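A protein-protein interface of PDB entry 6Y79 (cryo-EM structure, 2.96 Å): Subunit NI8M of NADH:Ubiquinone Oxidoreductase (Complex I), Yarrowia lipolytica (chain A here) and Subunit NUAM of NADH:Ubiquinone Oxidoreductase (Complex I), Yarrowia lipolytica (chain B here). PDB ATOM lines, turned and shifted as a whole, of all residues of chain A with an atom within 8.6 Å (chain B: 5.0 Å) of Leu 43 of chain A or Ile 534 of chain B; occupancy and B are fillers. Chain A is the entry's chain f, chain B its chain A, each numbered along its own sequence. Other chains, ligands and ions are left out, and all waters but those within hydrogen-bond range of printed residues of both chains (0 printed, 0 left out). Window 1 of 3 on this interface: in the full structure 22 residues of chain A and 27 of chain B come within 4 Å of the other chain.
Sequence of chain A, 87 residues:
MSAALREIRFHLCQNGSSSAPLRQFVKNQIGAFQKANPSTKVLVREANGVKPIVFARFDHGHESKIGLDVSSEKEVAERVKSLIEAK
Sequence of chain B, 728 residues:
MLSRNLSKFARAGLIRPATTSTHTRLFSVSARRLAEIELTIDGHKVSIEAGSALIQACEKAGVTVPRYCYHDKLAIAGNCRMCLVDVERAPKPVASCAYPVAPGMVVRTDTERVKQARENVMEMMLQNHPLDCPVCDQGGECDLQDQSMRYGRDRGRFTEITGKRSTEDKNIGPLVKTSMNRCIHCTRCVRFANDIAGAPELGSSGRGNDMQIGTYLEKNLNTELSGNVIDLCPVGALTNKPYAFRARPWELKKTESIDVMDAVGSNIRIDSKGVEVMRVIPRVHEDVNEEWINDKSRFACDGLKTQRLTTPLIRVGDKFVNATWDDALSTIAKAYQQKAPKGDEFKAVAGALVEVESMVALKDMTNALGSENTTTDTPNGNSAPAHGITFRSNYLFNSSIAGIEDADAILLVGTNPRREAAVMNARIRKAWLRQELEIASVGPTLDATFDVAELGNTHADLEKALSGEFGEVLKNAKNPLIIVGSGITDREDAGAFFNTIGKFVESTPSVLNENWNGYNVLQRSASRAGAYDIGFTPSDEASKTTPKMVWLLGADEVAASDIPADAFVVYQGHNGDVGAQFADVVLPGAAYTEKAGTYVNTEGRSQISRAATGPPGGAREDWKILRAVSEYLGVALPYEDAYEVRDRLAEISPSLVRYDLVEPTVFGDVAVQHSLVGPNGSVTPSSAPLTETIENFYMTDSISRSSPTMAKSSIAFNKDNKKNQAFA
The backbone carbonyl oxygen (O) of Ile 389 of chain B sits at hydrogen-bond distance from the guanidinium group (NH2) of Arg 45 of chain A.
The guanidinium group (NH1) of Arg 45 of chain A is in hydrogen-bond range of the backbone carbonyl oxygen (O) of Asp 533 of chain B.
The guanidinium group of Arg 45 of chain A is in hydrogen-bond range of the backbone carbonyl oxygen of Tyr 532 of chain B, at 2.8 Å.
A ring nitrogen (NE2) of His 11 of chain A is in hydrogen-bond range of the backbone carbonyl oxygen of Ile 652 of chain B.
N of Leu 12 of chain A sits at hydrogen-bond distance from O of Arg 45 of chain A (3.0 Å).
O of Arg 9 of chain A lies within hydrogen-bond range of N of Phe 55 of chain A, at 2.9 Å.
The backbone NH (N) of Phe 10 of chain A sits at hydrogen-bond distance from the backbone carbonyl oxygen (O) of Leu 43 of chain A (2.9 Å).
O of Ile 53 of chain A is in hydrogen-bond range of N of His 11 of chain A.
The backbone carbonyl oxygen (O) of Ile 8 of chain A lies within hydrogen-bond range of the backbone NH (N) of Leu 43 of chain A, at 2.9 Å.
OE2 of Glu 7 of chain A lies within salt-bridge range of NH2 of Arg 9 of chain A, at 3.8 Å.
Ile 652 of chain B touches Arg 9 of chain A.
Thr 390 of chain B touches Val 42 of chain A.
Leu 43 of chain A touches Ile 389 of chain B (CD2 to CG2, 3.6 Å).
CD1 of Leu 43 of chain A touches O of Ile 534 of chain B, at 3.6 Å.
Phe 10 of chain A touches none of the printed residues of chain B.
Gln 34 of chain A touches none of the printed residues of chain B.
Leu 43 of chain A touches just these residues of chain B: Ile 389 (3.6 Å) and Ile 534 (3.6 Å).
Of the printed residues of chain A, Ile 389 of chain B touches Leu 43 (3.6 Å) and Arg 45 (3.4 Å).
Of the printed residues of chain A, Thr 390 of chain B touches Val 42.
Printed residues of chain A within 4 Å of Tyr 532 of chain B: Arg 45 (2.8 Å).
No residue of chain A comes within 4 Å of Gly 535 of chain B.
The nearest residue of chain A that does not touch Ile 534 of chain B is Arg 45 of chain A (4.5 Å).
Hydrophobic or aromatic side chains of chain A within 4 Å of the printed part of chain B: His 11 and Leu 43.
Of the 14 printed residues of chain B, 6 touch a printed residue of chain A.
Printed residues of chain B that touch a printed residue of chain A: Ile 389, Thr 390, Tyr 532, Asp 533, Ile 534 and Ile 652.
Hydrophobic or aromatic side chains of chain B that line the printed part of chain A: Ile 389.
Among the printed residues, no Asp or Glu carboxylate lies within 4 Å of a Lys or Arg side-chain nitrogen of the other chain.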
ATOM      1  N   GLU A   7      15.490   0.396 -21.321  1.00  0.00           N
ATOM      2  CA  GLU A   7      15.481  -0.960 -21.881  1.00  0.00           C
ATOM      3  C   GLU A   7      15.397  -0.909 -23.403  1.00  0.00           C
ATOM      4  O   GLU A   7      15.083   0.129 -23.987  1.00  0.00           O
ATOM      5  CB  GLU A   7      14.314  -1.831 -21.334  1.00  0.00           C
ATOM      6  CG  GLU A   7      12.876  -1.377 -21.634  1.00  0.00           C
ATOM      7  CD  GLU A   7      12.348  -1.986 -22.921  1.00  0.00           C
ATOM      8  OE1 GLU A   7      12.929  -2.994 -23.377  1.00  0.00           O
ATOM      9  OE2 GLU A   7      11.363  -1.459 -23.472  1.00  0.00           O
ATOM     10  N   ILE A   8      15.653  -2.052 -24.043  1.00  0.00           N
ATOM     11  CA  ILE A   8      15.764  -2.119 -25.496  1.00  0.00           C
ATOM     12  C   ILE A   8      14.862  -3.235 -26.028  1.00  0.00           C
ATOM     13  O   ILE A   8      14.694  -4.288 -25.399  1.00  0.00           O
ATOM     14  CB  ILE A   8      17.249  -2.302 -25.917  1.00  0.00           C
ATOM     15  CG1 ILE A   8      17.426  -2.154 -27.424  1.00  0.00           C
ATOM     16  CG2 ILE A   8      17.827  -3.618 -25.452  1.00  0.00           C
ATOM     17  CD1 ILE A   8      18.818  -1.816 -27.850  1.00  0.00           C
ATOM     18  N   ARG A   9      14.236  -2.983 -27.176  1.00  0.00           N
ATOM     19  CA  ARG A   9      13.302  -3.941 -27.755  1.00  0.00           C
ATOM     20  C   ARG A   9      13.428  -3.917 -29.268  1.00  0.00           C
ATOM     21  O   ARG A   9      13.600  -2.854 -29.862  1.00  0.00           O
ATOM     22  CB  ARG A   9      11.855  -3.619 -27.365  1.00  0.00           C
ATOM     23  CG  ARG A   9      11.392  -2.215 -27.708  1.00  0.00           C
ATOM     24  CD  ARG A   9       9.977  -1.968 -27.260  1.00  0.00           C
ATOM     25  NE  ARG A   9       9.429  -0.792 -27.918  1.00  0.00           N
ATOM     26  CZ  ARG A   9       9.581   0.447 -27.473  1.00  0.00           C
ATOM     27  NH1 ARG A   9       9.052   1.458 -28.143  1.00  0.00           N
ATOM     28  NH2 ARG A   9      10.260   0.675 -26.360  1.00  0.00           N
ATOM     29  N   PHE A  10      13.291  -5.081 -29.907  1.00  0.00           N
ATOM     30  CA  PHE A  10      13.343  -5.087 -31.367  1.00  0.00           C
ATOM     31  C   PHE A  10      12.367  -6.062 -31.982  1.00  0.00           C
ATOM     32  O   PHE A  10      11.834  -6.955 -31.319  1.00  0.00           O
ATOM     33  CB  PHE A  10      14.722  -5.391 -31.944  1.00  0.00           C
ATOM     34  CG  PHE A  10      15.386  -6.599 -31.418  1.00  0.00           C
ATOM     35  CD1 PHE A  10      16.123  -6.584 -30.236  1.00  0.00           C
ATOM     36  CD2 PHE A  10      15.405  -7.717 -32.192  1.00  0.00           C
ATOM     37  CE1 PHE A  10      16.777  -7.728 -29.815  1.00  0.00           C
ATOM     38  CE2 PHE A  10      16.066  -8.839 -31.792  1.00  0.00           C
ATOM     39  CZ  PHE A  10      16.740  -8.861 -30.607  1.00  0.00           C
ATOM     40  N   HIS A  11      12.200  -5.900 -33.295  1.00  0.00           N
ATOM     41  CA  HIS A  11      11.073  -6.454 -34.020  1.00  0.00           C
ATOM     42  C   HIS A  11      11.519  -7.079 -35.324  1.00  0.00           C
ATOM     43  O   HIS A  11      12.180  -6.429 -36.150  1.00  0.00           O
ATOM     44  CB  HIS A  11      10.034  -5.371 -34.276  1.00  0.00           C
ATOM     45  CG  HIS A  11       9.460  -4.826 -33.017  1.00  0.00           C
ATOM     46  ND1 HIS A  11       8.842  -5.638 -32.094  1.00  0.00           N
ATOM     47  CD2 HIS A  11       9.451  -3.580 -32.493  1.00  0.00           C
ATOM     48  CE1 HIS A  11       8.462  -4.912 -31.062  1.00  0.00           C
ATOM     49  NE2 HIS A  11       8.812  -3.658 -31.280  1.00  0.00           N
ATOM     50  N   LEU A  12      11.102  -8.335 -35.492  1.00  0.00           N
ATOM     51  CA  LEU A  12      11.426  -9.177 -36.630  1.00  0.00           C
ATOM     52  C   LEU A  12      10.150  -9.504 -37.389  1.00  0.00           C
ATOM     53  O   LEU A  12       9.035  -9.346 -36.883  1.00  0.00           O
ATOM     54  CB  LEU A  12      12.071 -10.513 -36.216  1.00  0.00           C
ATOM     55  CG  LEU A  12      13.403 -10.614 -35.546  1.00  0.00           C
ATOM     56  CD1 LEU A  12      13.271 -10.444 -34.048  1.00  0.00           C
ATOM     57  CD2 LEU A  12      14.021 -11.972 -35.842  1.00  0.00           C
ATOM     58  N   ILE A  30      22.065 -13.016 -27.721  1.00  0.00           N
ATOM     59  CA  ILE A  30      21.188 -12.715 -26.574  1.00  0.00           C
ATOM     60  C   ILE A  30      21.959 -12.753 -25.246  1.00  0.00           C
ATOM     61  O   ILE A  30      21.963 -11.774 -24.474  1.00  0.00           O
ATOM     62  CB  ILE A  30      19.998 -13.682 -26.516  1.00  0.00           C
ATOM     63  CG1 ILE A  30      19.161 -13.611 -27.771  1.00  0.00           C
ATOM     64  CG2 ILE A  30      19.136 -13.321 -25.322  1.00  0.00           C
ATOM     65  CD1 ILE A  30      18.571 -12.267 -28.015  1.00  0.00           C
ATOM     66  N   PHE A  33      24.536 -10.005 -24.753  1.00  0.00           N
ATOM     67  CA  PHE A  33      24.018  -8.670 -24.490  1.00  0.00           C
ATOM     68  C   PHE A  33      23.445  -8.538 -23.085  1.00  0.00           C
ATOM     69  O   PHE A  33      23.470  -7.435 -22.525  1.00  0.00           O
ATOM     70  CB  PHE A  33      22.956  -8.269 -25.508  1.00  0.00           C
ATOM     71  CG  PHE A  33      22.499  -6.852 -25.342  1.00  0.00           C
ATOM     72  CD1 PHE A  33      23.334  -5.808 -25.689  1.00  0.00           C
ATOM     73  CD2 PHE A  33      21.270  -6.562 -24.779  1.00  0.00           C
ATOM     74  CE1 PHE A  33      22.939  -4.505 -25.510  1.00  0.00           C
ATOM     75  CE2 PHE A  33      20.869  -5.257 -24.597  1.00  0.00           C
ATOM     76  CZ  PHE A  33      21.703  -4.227 -24.967  1.00  0.00           C
ATOM     77  N   GLN A  34      22.928  -9.624 -22.499  1.00  0.00           N
ATOM     78  CA  GLN A  34      22.279  -9.456 -21.196  1.00  0.00           C
ATOM     79  C   GLN A  34      23.291  -9.149 -20.089  1.00  0.00           C
ATOM     80  O   GLN A  34      23.027  -8.314 -19.216  1.00  0.00           O
ATOM     81  CB  GLN A  34      21.435 -10.677 -20.834  1.00  0.00           C
ATOM     82  CG  GLN A  34      20.618 -10.491 -19.537  1.00  0.00           C
ATOM     83  CD  GLN A  34      19.883  -9.144 -19.450  1.00  0.00           C
ATOM     84  OE1 GLN A  34      20.271  -8.252 -18.691  1.00  0.00           O
ATOM     85  NE2 GLN A  34      18.806  -9.009 -20.204  1.00  0.00           N
ATOM     86  N   THR A  40      19.418  -3.546 -17.975  1.00  0.00           N
ATOM     87  CA  THR A  40      18.612  -3.172 -19.127  1.00  0.00           C
ATOM     88  C   THR A  40      17.829  -4.404 -19.610  1.00  0.00           C
ATOM     89  O   THR A  40      18.402  -5.473 -19.855  1.00  0.00           O
ATOM     90  CB  THR A  40      19.556  -2.599 -20.209  1.00  0.00           C
ATOM     91  OG1 THR A  40      20.045  -1.322 -19.770  1.00  0.00           O
ATOM     92  CG2 THR A  40      18.926  -2.493 -21.604  1.00  0.00           C
ATOM     93  N   LYS A  41      16.524  -4.255 -19.793  1.00  0.00           N
ATOM     94  CA  LYS A  41      15.659  -5.362 -20.182  1.00  0.00           C
ATOM     95  C   LYS A  41      15.672  -5.458 -21.700  1.00  0.00           C
ATOM     96  O   LYS A  41      15.919  -4.461 -22.385  1.00  0.00           O
ATOM     97  CB  LYS A  41      14.229  -5.156 -19.666  1.00  0.00           C
ATOM     98  CG  LYS A  41      14.160  -4.870 -18.176  1.00  0.00           C
ATOM     99  CD  LYS A  41      12.770  -4.421 -17.749  1.00  0.00           C
ATOM    100  CE  LYS A  41      12.785  -3.970 -16.298  1.00  0.00           C
ATOM    101  NZ  LYS A  41      11.436  -3.547 -15.860  1.00  0.00           N
ATOM    102  N   VAL A  42      15.468  -6.657 -22.216  1.00  0.00           N
ATOM    103  CA  VAL A  42      15.388  -6.885 -23.644  1.00  0.00           C
ATOM    104  C   VAL A  42      14.005  -7.438 -23.964  1.00  0.00           C
ATOM    105  O   VAL A  42      13.504  -8.351 -23.307  1.00  0.00           O
ATOM    106  CB  VAL A  42      16.504  -7.844 -24.134  1.00  0.00           C
ATOM    107  CG1 VAL A  42      16.394  -8.115 -25.636  1.00  0.00           C
ATOM    108  CG2 VAL A  42      17.866  -7.274 -23.814  1.00  0.00           C
ATOM    109  N   LEU A  43      13.364  -6.867 -24.983  1.00  0.00           N
ATOM    110  CA  LEU A  43      12.078  -7.385 -25.447  1.00  0.00           C
ATOM    111  C   LEU A  43      12.238  -7.698 -26.923  1.00  0.00           C
ATOM    112  O   LEU A  43      12.609  -6.819 -27.703  1.00  0.00           O
ATOM    113  CB  LEU A  43      10.945  -6.386 -25.243  1.00  0.00           C
ATOM    114  CG  LEU A  43      10.856  -5.485 -24.020  1.00  0.00           C
ATOM    115  CD1 LEU A  43       9.591  -4.666 -24.113  1.00  0.00           C
ATOM    116  CD2 LEU A  43      10.860  -6.282 -22.749  1.00  0.00           C
ATOM    117  N   VAL A  44      11.978  -8.936 -27.311  1.00  0.00           N
ATOM    118  CA  VAL A  44      12.092  -9.346 -28.701  1.00  0.00           C
ATOM    119  C   VAL A  44      10.698  -9.763 -29.172  1.00  0.00           C
ATOM    120  O   VAL A  44       9.983 -10.491 -28.471  1.00  0.00           O
ATOM    121  CB  VAL A  44      13.177 -10.436 -28.867  1.00  0.00           C
ATOM    122  CG1 VAL A  44      12.864 -11.745 -28.137  1.00  0.00           C
ATOM    123  CG2 VAL A  44      13.499 -10.678 -30.302  1.00  0.00           C
ATOM    124  N   ARG A  45      10.262  -9.220 -30.306  1.00  0.00           N
ATOM    125  CA  ARG A  45       8.895  -9.470 -30.739  1.00  0.00           C
ATOM    126  C   ARG A  45       8.846  -9.671 -32.245  1.00  0.00           C
ATOM    127  O   ARG A  45       9.655  -9.122 -33.001  1.00  0.00           O
ATOM    128  CB  ARG A  45       7.936  -8.341 -30.331  1.00  0.00           C
ATOM    129  CG  ARG A  45       7.341  -8.494 -28.940  1.00  0.00           C
ATOM    130  CD  ARG A  45       8.112  -7.657 -27.949  1.00  0.00           C
ATOM    131  NE  ARG A  45       7.591  -7.742 -26.587  1.00  0.00           N
ATOM    132  CZ  ARG A  45       7.902  -8.702 -25.722  1.00  0.00           C
ATOM    133  NH1 ARG A  45       7.389  -8.686 -24.505  1.00  0.00           N
ATOM    134  NH2 ARG A  45       8.725  -9.677 -26.067  1.00  0.00           N
ATOM    135  N   GLU A  46       7.845 -10.442 -32.665  1.00  0.00           N
ATOM    136  CA  GLU A  46       7.816 -11.101 -33.965  1.00  0.00           C
ATOM    137  C   GLU A  46       6.411 -11.048 -34.537  1.00  0.00           C
ATOM    138  O   GLU A  46       5.443 -11.385 -33.844  1.00  0.00           O
ATOM    139  CB  GLU A  46       8.259 -12.566 -33.850  1.00  0.00           C
ATOM    140  CG  GLU A  46       9.711 -12.796 -33.535  1.00  0.00           C
ATOM    141  CD  GLU A  46       9.988 -12.766 -32.020  1.00  0.00           C
ATOM    142  OE1 GLU A  46       9.027 -12.860 -31.254  1.00  0.00           O
ATOM    143  OE2 GLU A  46      11.148 -12.548 -31.649  1.00  0.00           O
ATOM    144  N   ILE A  53      13.409  -3.690 -36.870  1.00  0.00           N
ATOM    145  CA  ILE A  53      13.583  -2.351 -36.290  1.00  0.00           C
ATOM    146  C   ILE A  53      13.950  -2.534 -34.819  1.00  0.00           C
ATOM    147  O   ILE A  53      13.394  -3.409 -34.161  1.00  0.00           O
ATOM    148  CB  ILE A  53      12.309  -1.487 -36.487  1.00  0.00           C
ATOM    149  CG1 ILE A  53      12.176  -0.993 -37.927  1.00  0.00           C
ATOM    150  CG2 ILE A  53      12.300  -0.260 -35.588  1.00  0.00           C
ATOM    151  CD1 ILE A  53      10.780  -0.547 -38.251  1.00  0.00           C
ATOM    152  N   VAL A  54      14.882  -1.739 -34.275  1.00  0.00           N
ATOM    153  CA  VAL A  54      15.067  -1.734 -32.821  1.00  0.00           C
ATOM    154  C   VAL A  54      14.776  -0.342 -32.280  1.00  0.00           C
ATOM    155  O   VAL A  54      15.047   0.669 -32.942  1.00  0.00           O
ATOM    156  CB  VAL A  54      16.465  -2.253 -32.388  1.00  0.00           C
ATOM    157  CG1 VAL A  54      17.593  -1.316 -32.620  1.00  0.00           C
ATOM    158  CG2 VAL A  54      16.580  -2.563 -30.905  1.00  0.00           C
ATOM    159  N   PHE A  55      14.085  -0.320 -31.148  1.00  0.00           N
ATOM    160  CA  PHE A  55      13.874   0.843 -30.311  1.00  0.00           C
ATOM    161  C   PHE A  55      14.711   0.668 -29.056  1.00  0.00           C
ATOM    162  O   PHE A  55      14.861  -0.455 -28.556  1.00  0.00           O
ATOM    163  CB  PHE A  55      12.405   0.959 -29.910  1.00  0.00           C
ATOM    164  CG  PHE A  55      11.465   1.180 -31.051  1.00  0.00           C
ATOM    165  CD1 PHE A  55      10.953   0.115 -31.775  1.00  0.00           C
ATOM    166  CD2 PHE A  55      11.060   2.459 -31.369  1.00  0.00           C
ATOM    167  CE1 PHE A  55      10.079   0.328 -32.813  1.00  0.00           C
ATOM    168  CE2 PHE A  55      10.188   2.678 -32.401  1.00  0.00           C
ATOM    169  CZ  PHE A  55       9.697   1.613 -33.128  1.00  0.00           C
ATOM    170  N   ARG A  57      14.976   2.707 -25.138  1.00  0.00           N
ATOM    171  CA  ARG A  57      14.347   3.640 -24.219  1.00  0.00           C
ATOM    172  C   ARG A  57      15.398   4.030 -23.200  1.00  0.00           C
ATOM    173  O   ARG A  57      15.847   3.174 -22.431  1.00  0.00           O
ATOM    174  CB  ARG A  57      13.160   2.972 -23.515  1.00  0.00           C
ATOM    175  CG  ARG A  57      12.025   3.873 -23.085  1.00  0.00           C
ATOM    176  CD  ARG A  57      12.097   4.366 -21.630  1.00  0.00           C
ATOM    177  NE  ARG A  57      12.342   3.361 -20.588  1.00  0.00           N
ATOM    178  CZ  ARG A  57      11.451   2.467 -20.160  1.00  0.00           C
ATOM    179  NH1 ARG A  57      11.771   1.626 -19.186  1.00  0.00           N
ATOM    180  NH2 ARG A  57      10.250   2.394 -20.716  1.00  0.00           N
ATOM    181  N   VAL B 356      -4.805  -3.084 -22.509  1.00  0.00           N
ATOM    182  CA  VAL B 356      -3.431  -2.949 -22.979  1.00  0.00           C
ATOM    183  C   VAL B 356      -3.079  -1.480 -23.191  1.00  0.00           C
ATOM    184  O   VAL B 356      -1.986  -1.040 -22.826  1.00  0.00           O
ATOM    185  CB  VAL B 356      -3.225  -3.781 -24.259  1.00  0.00           C
ATOM    186  CG1 VAL B 356      -1.860  -3.556 -24.833  1.00  0.00           C
ATOM    187  CG2 VAL B 356      -3.391  -5.258 -23.954  1.00  0.00           C
ATOM    188  N   MET B 359      -2.333   0.138 -19.990  1.00  0.00           N
ATOM    189  CA  MET B 359      -0.969  -0.209 -19.601  1.00  0.00           C
ATOM    190  C   MET B 359       0.075   0.573 -20.398  1.00  0.00           C
ATOM    191  O   MET B 359       1.137   0.895 -19.854  1.00  0.00           O
ATOM    192  CB  MET B 359      -0.739  -1.711 -19.737  1.00  0.00           C
ATOM    193  CG  MET B 359      -1.464  -2.511 -18.682  1.00  0.00           C
ATOM    194  SD  MET B 359      -1.083  -4.270 -18.676  1.00  0.00           S
ATOM    195  CE  MET B 359      -2.030  -4.856 -20.075  1.00  0.00           C
ATOM    196  N   VAL B 360      -0.213   0.880 -21.672  1.00  0.00           N
ATOM    197  CA  VAL B 360       0.645   1.765 -22.468  1.00  0.00           C
ATOM    198  C   VAL B 360       0.759   3.125 -21.799  1.00  0.00           C
ATOM    199  O   VAL B 360       1.862   3.657 -21.604  1.00  0.00           O
ATOM    200  CB  VAL B 360       0.102   1.923 -23.903  1.00  0.00           C
ATOM    201  CG1 VAL B 360       0.954   2.904 -24.688  1.00  0.00           C
ATOM    202  CG2 VAL B 360       0.023   0.616 -24.636  1.00  0.00           C
ATOM    203  N   LYS B 363       2.708   2.797 -18.310  1.00  0.00           N
ATOM    204  CA  LYS B 363       4.133   2.548 -18.480  1.00  0.00           C
ATOM    205  C   LYS B 363       4.848   3.770 -19.049  1.00  0.00           C
ATOM    206  O   LYS B 363       5.942   4.128 -18.585  1.00  0.00           O
ATOM    207  CB  LYS B 363       4.330   1.330 -19.381  1.00  0.00           C
ATOM    208  CG  LYS B 363       5.761   0.910 -19.488  1.00  0.00           C
ATOM    209  CD  LYS B 363       5.988  -0.327 -20.313  1.00  0.00           C
ATOM    210  CE  LYS B 363       7.476  -0.622 -20.331  1.00  0.00           C
ATOM    211  NZ  LYS B 363       7.824  -1.813 -21.137  1.00  0.00           N
ATOM    212  N   ILE B 389      10.506 -12.032 -19.798  1.00  0.00           N
ATOM    213  CA  ILE B 389       9.763 -11.093 -20.634  1.00  0.00           C
ATOM    214  C   ILE B 389      10.337 -11.109 -22.038  1.00  0.00           C
ATOM    215  O   ILE B 389       9.614 -10.965 -23.036  1.00  0.00           O
ATOM    216  CB  ILE B 389       9.821  -9.691 -20.006  1.00  0.00           C
ATOM    217  CG1 ILE B 389       9.277  -9.778 -18.594  1.00  0.00           C
ATOM    218  CG2 ILE B 389       9.032  -8.671 -20.816  1.00  0.00           C
ATOM    219  CD1 ILE B 389       7.852 -10.240 -18.530  1.00  0.00           C
ATOM    220  N   THR B 390      11.660 -11.248 -22.117  1.00  0.00           N
ATOM    221  CA  THR B 390      12.363 -11.754 -23.283  1.00  0.00           C
ATOM    222  C   THR B 390      11.672 -12.995 -23.826  1.00  0.00           C
ATOM    223  O   THR B 390      11.252 -13.860 -23.050  1.00  0.00           O
ATOM    224  CB  THR B 390      13.783 -12.138 -22.875  1.00  0.00           C
ATOM    225  OG1 THR B 390      13.721 -13.322 -22.070  1.00  0.00           O
ATOM    226  CG2 THR B 390      14.388 -11.061 -22.010  1.00  0.00           C
ATOM    227  N   GLY B 530      -0.777  -9.436 -21.678  1.00  0.00           N
ATOM    228  CA  GLY B 530      -0.548  -8.142 -22.304  1.00  0.00           C
ATOM    229  C   GLY B 530       0.510  -7.329 -21.583  1.00  0.00           C
ATOM    230  O   GLY B 530       1.298  -6.615 -22.213  1.00  0.00           O
ATOM    231  N   ALA B 531       0.558  -7.450 -20.253  1.00  0.00           N
ATOM    232  CA  ALA B 531       1.598  -6.805 -19.461  1.00  0.00           C
ATOM    233  C   ALA B 531       2.972  -7.384 -19.768  1.00  0.00           C
ATOM    234  O   ALA B 531       3.966  -6.649 -19.841  1.00  0.00           O
ATOM    235  CB  ALA B 531       1.277  -6.955 -17.974  1.00  0.00           C
ATOM    236  N   TYR B 532       3.051  -8.687 -19.980  1.00  0.00           N
ATOM    237  CA  TYR B 532       4.337  -9.263 -20.322  1.00  0.00           C
ATOM    238  C   TYR B 532       4.689  -9.052 -21.791  1.00  0.00           C
ATOM    239  O   TYR B 532       5.870  -9.140 -22.146  1.00  0.00           O
ATOM    240  CB  TYR B 532       4.355 -10.751 -19.960  1.00  0.00           C
ATOM    241  CG  TYR B 532       4.291 -11.073 -18.472  1.00  0.00           C
ATOM    242  CD1 TYR B 532       4.478 -10.090 -17.506  1.00  0.00           C
ATOM    243  CD2 TYR B 532       4.052 -12.372 -18.040  1.00  0.00           C
ATOM    244  CE1 TYR B 532       4.431 -10.390 -16.160  1.00  0.00           C
ATOM    245  CE2 TYR B 532       3.999 -12.681 -16.694  1.00  0.00           C
ATOM    246  CZ  TYR B 532       4.189 -11.684 -15.761  1.00  0.00           C
ATOM    247  OH  TYR B 532       4.138 -11.985 -14.420  1.00  0.00           O
ATOM    248  N   ASP B 533       3.700  -8.774 -22.648  1.00  0.00           N
ATOM    249  CA  ASP B 533       3.992  -8.309 -24.002  1.00  0.00           C
ATOM    250  C   ASP B 533       4.601  -6.921 -23.987  1.00  0.00           C
ATOM    251  O   ASP B 533       5.592  -6.658 -24.679  1.00  0.00           O
ATOM    252  CB  ASP B 533       2.726  -8.288 -24.855  1.00  0.00           C
ATOM    253  CG  ASP B 533       2.226  -9.666 -25.203  1.00  0.00           C
ATOM    254  OD1 ASP B 533       3.031 -10.609 -25.299  1.00  0.00           O
ATOM    255  OD2 ASP B 533       1.006  -9.797 -25.391  1.00  0.00           O
ATOM    256  N   ILE B 534       4.004  -6.016 -23.216  1.00  0.00           N
ATOM    257  CA  ILE B 534       4.452  -4.633 -23.215  1.00  0.00           C
ATOM    258  C   ILE B 534       5.741  -4.456 -22.416  1.00  0.00           C
ATOM    259  O   ILE B 534       6.472  -3.484 -22.638  1.00  0.00           O
ATOM    260  CB  ILE B 534       3.283  -3.763 -22.714  1.00  0.00           C
ATOM    261  CG1 ILE B 534       3.504  -2.280 -22.957  1.00  0.00           C
ATOM    262  CG2 ILE B 534       3.050  -3.936 -21.266  1.00  0.00           C
ATOM    263  CD1 ILE B 534       2.289  -1.480 -22.617  1.00  0.00           C
ATOM    264  N   GLY B 535       6.077  -5.391 -21.534  1.00  0.00           N
ATOM    265  CA  GLY B 535       7.262  -5.254 -20.714  1.00  0.00           C
ATOM    266  C   GLY B 535       6.981  -4.691 -19.347  1.00  0.00           C
ATOM    267  O   GLY B 535       7.889  -4.123 -18.726  1.00  0.00           O
ATOM    268  N   PHE B 536       5.748  -4.832 -18.871  1.00  0.00           N
ATOM    269  CA  PHE B 536       5.247  -4.278 -17.619  1.00  0.00           C
ATOM    270  C   PHE B 536       5.716  -5.174 -16.475  1.00  0.00           C
ATOM    271  O   PHE B 536       4.998  -6.049 -15.981  1.00  0.00           O
ATOM    272  CB  PHE B 536       3.732  -4.187 -17.716  1.00  0.00           C
ATOM    273  CG  PHE B 536       3.057  -3.569 -16.555  1.00  0.00           C
ATOM    274  CD1 PHE B 536       3.009  -2.199 -16.408  1.00  0.00           C
ATOM    275  CD2 PHE B 536       2.390  -4.361 -15.647  1.00  0.00           C
ATOM    276  CE1 PHE B 536       2.352  -1.638 -15.337  1.00  0.00           C
ATOM    277  CE2 PHE B 536       1.739  -3.813 -14.591  1.00  0.00           C
ATOM    278  CZ  PHE B 536       1.738  -2.447 -14.423  1.00  0.00           C
ATOM    279  N   ILE B 652       5.276  -0.492 -29.548  1.00  0.00           N
ATOM    280  CA  ILE B 652       5.638  -1.477 -28.535  1.00  0.00           C
ATOM    281  C   ILE B 652       5.852  -2.843 -29.186  1.00  0.00           C
ATOM    282  O   ILE B 652       6.958  -3.385 -29.155  1.00  0.00           O
ATOM    283  CB  ILE B 652       4.585  -1.547 -27.422  1.00  0.00           C
ATOM    284  CG1 ILE B 652       4.560  -0.265 -26.654  1.00  0.00           C
ATOM    285  CG2 ILE B 652       4.866  -2.736 -26.495  1.00  0.00           C
ATOM    286  CD1 ILE B 652       3.351  -0.086 -25.885  1.00  0.00           C
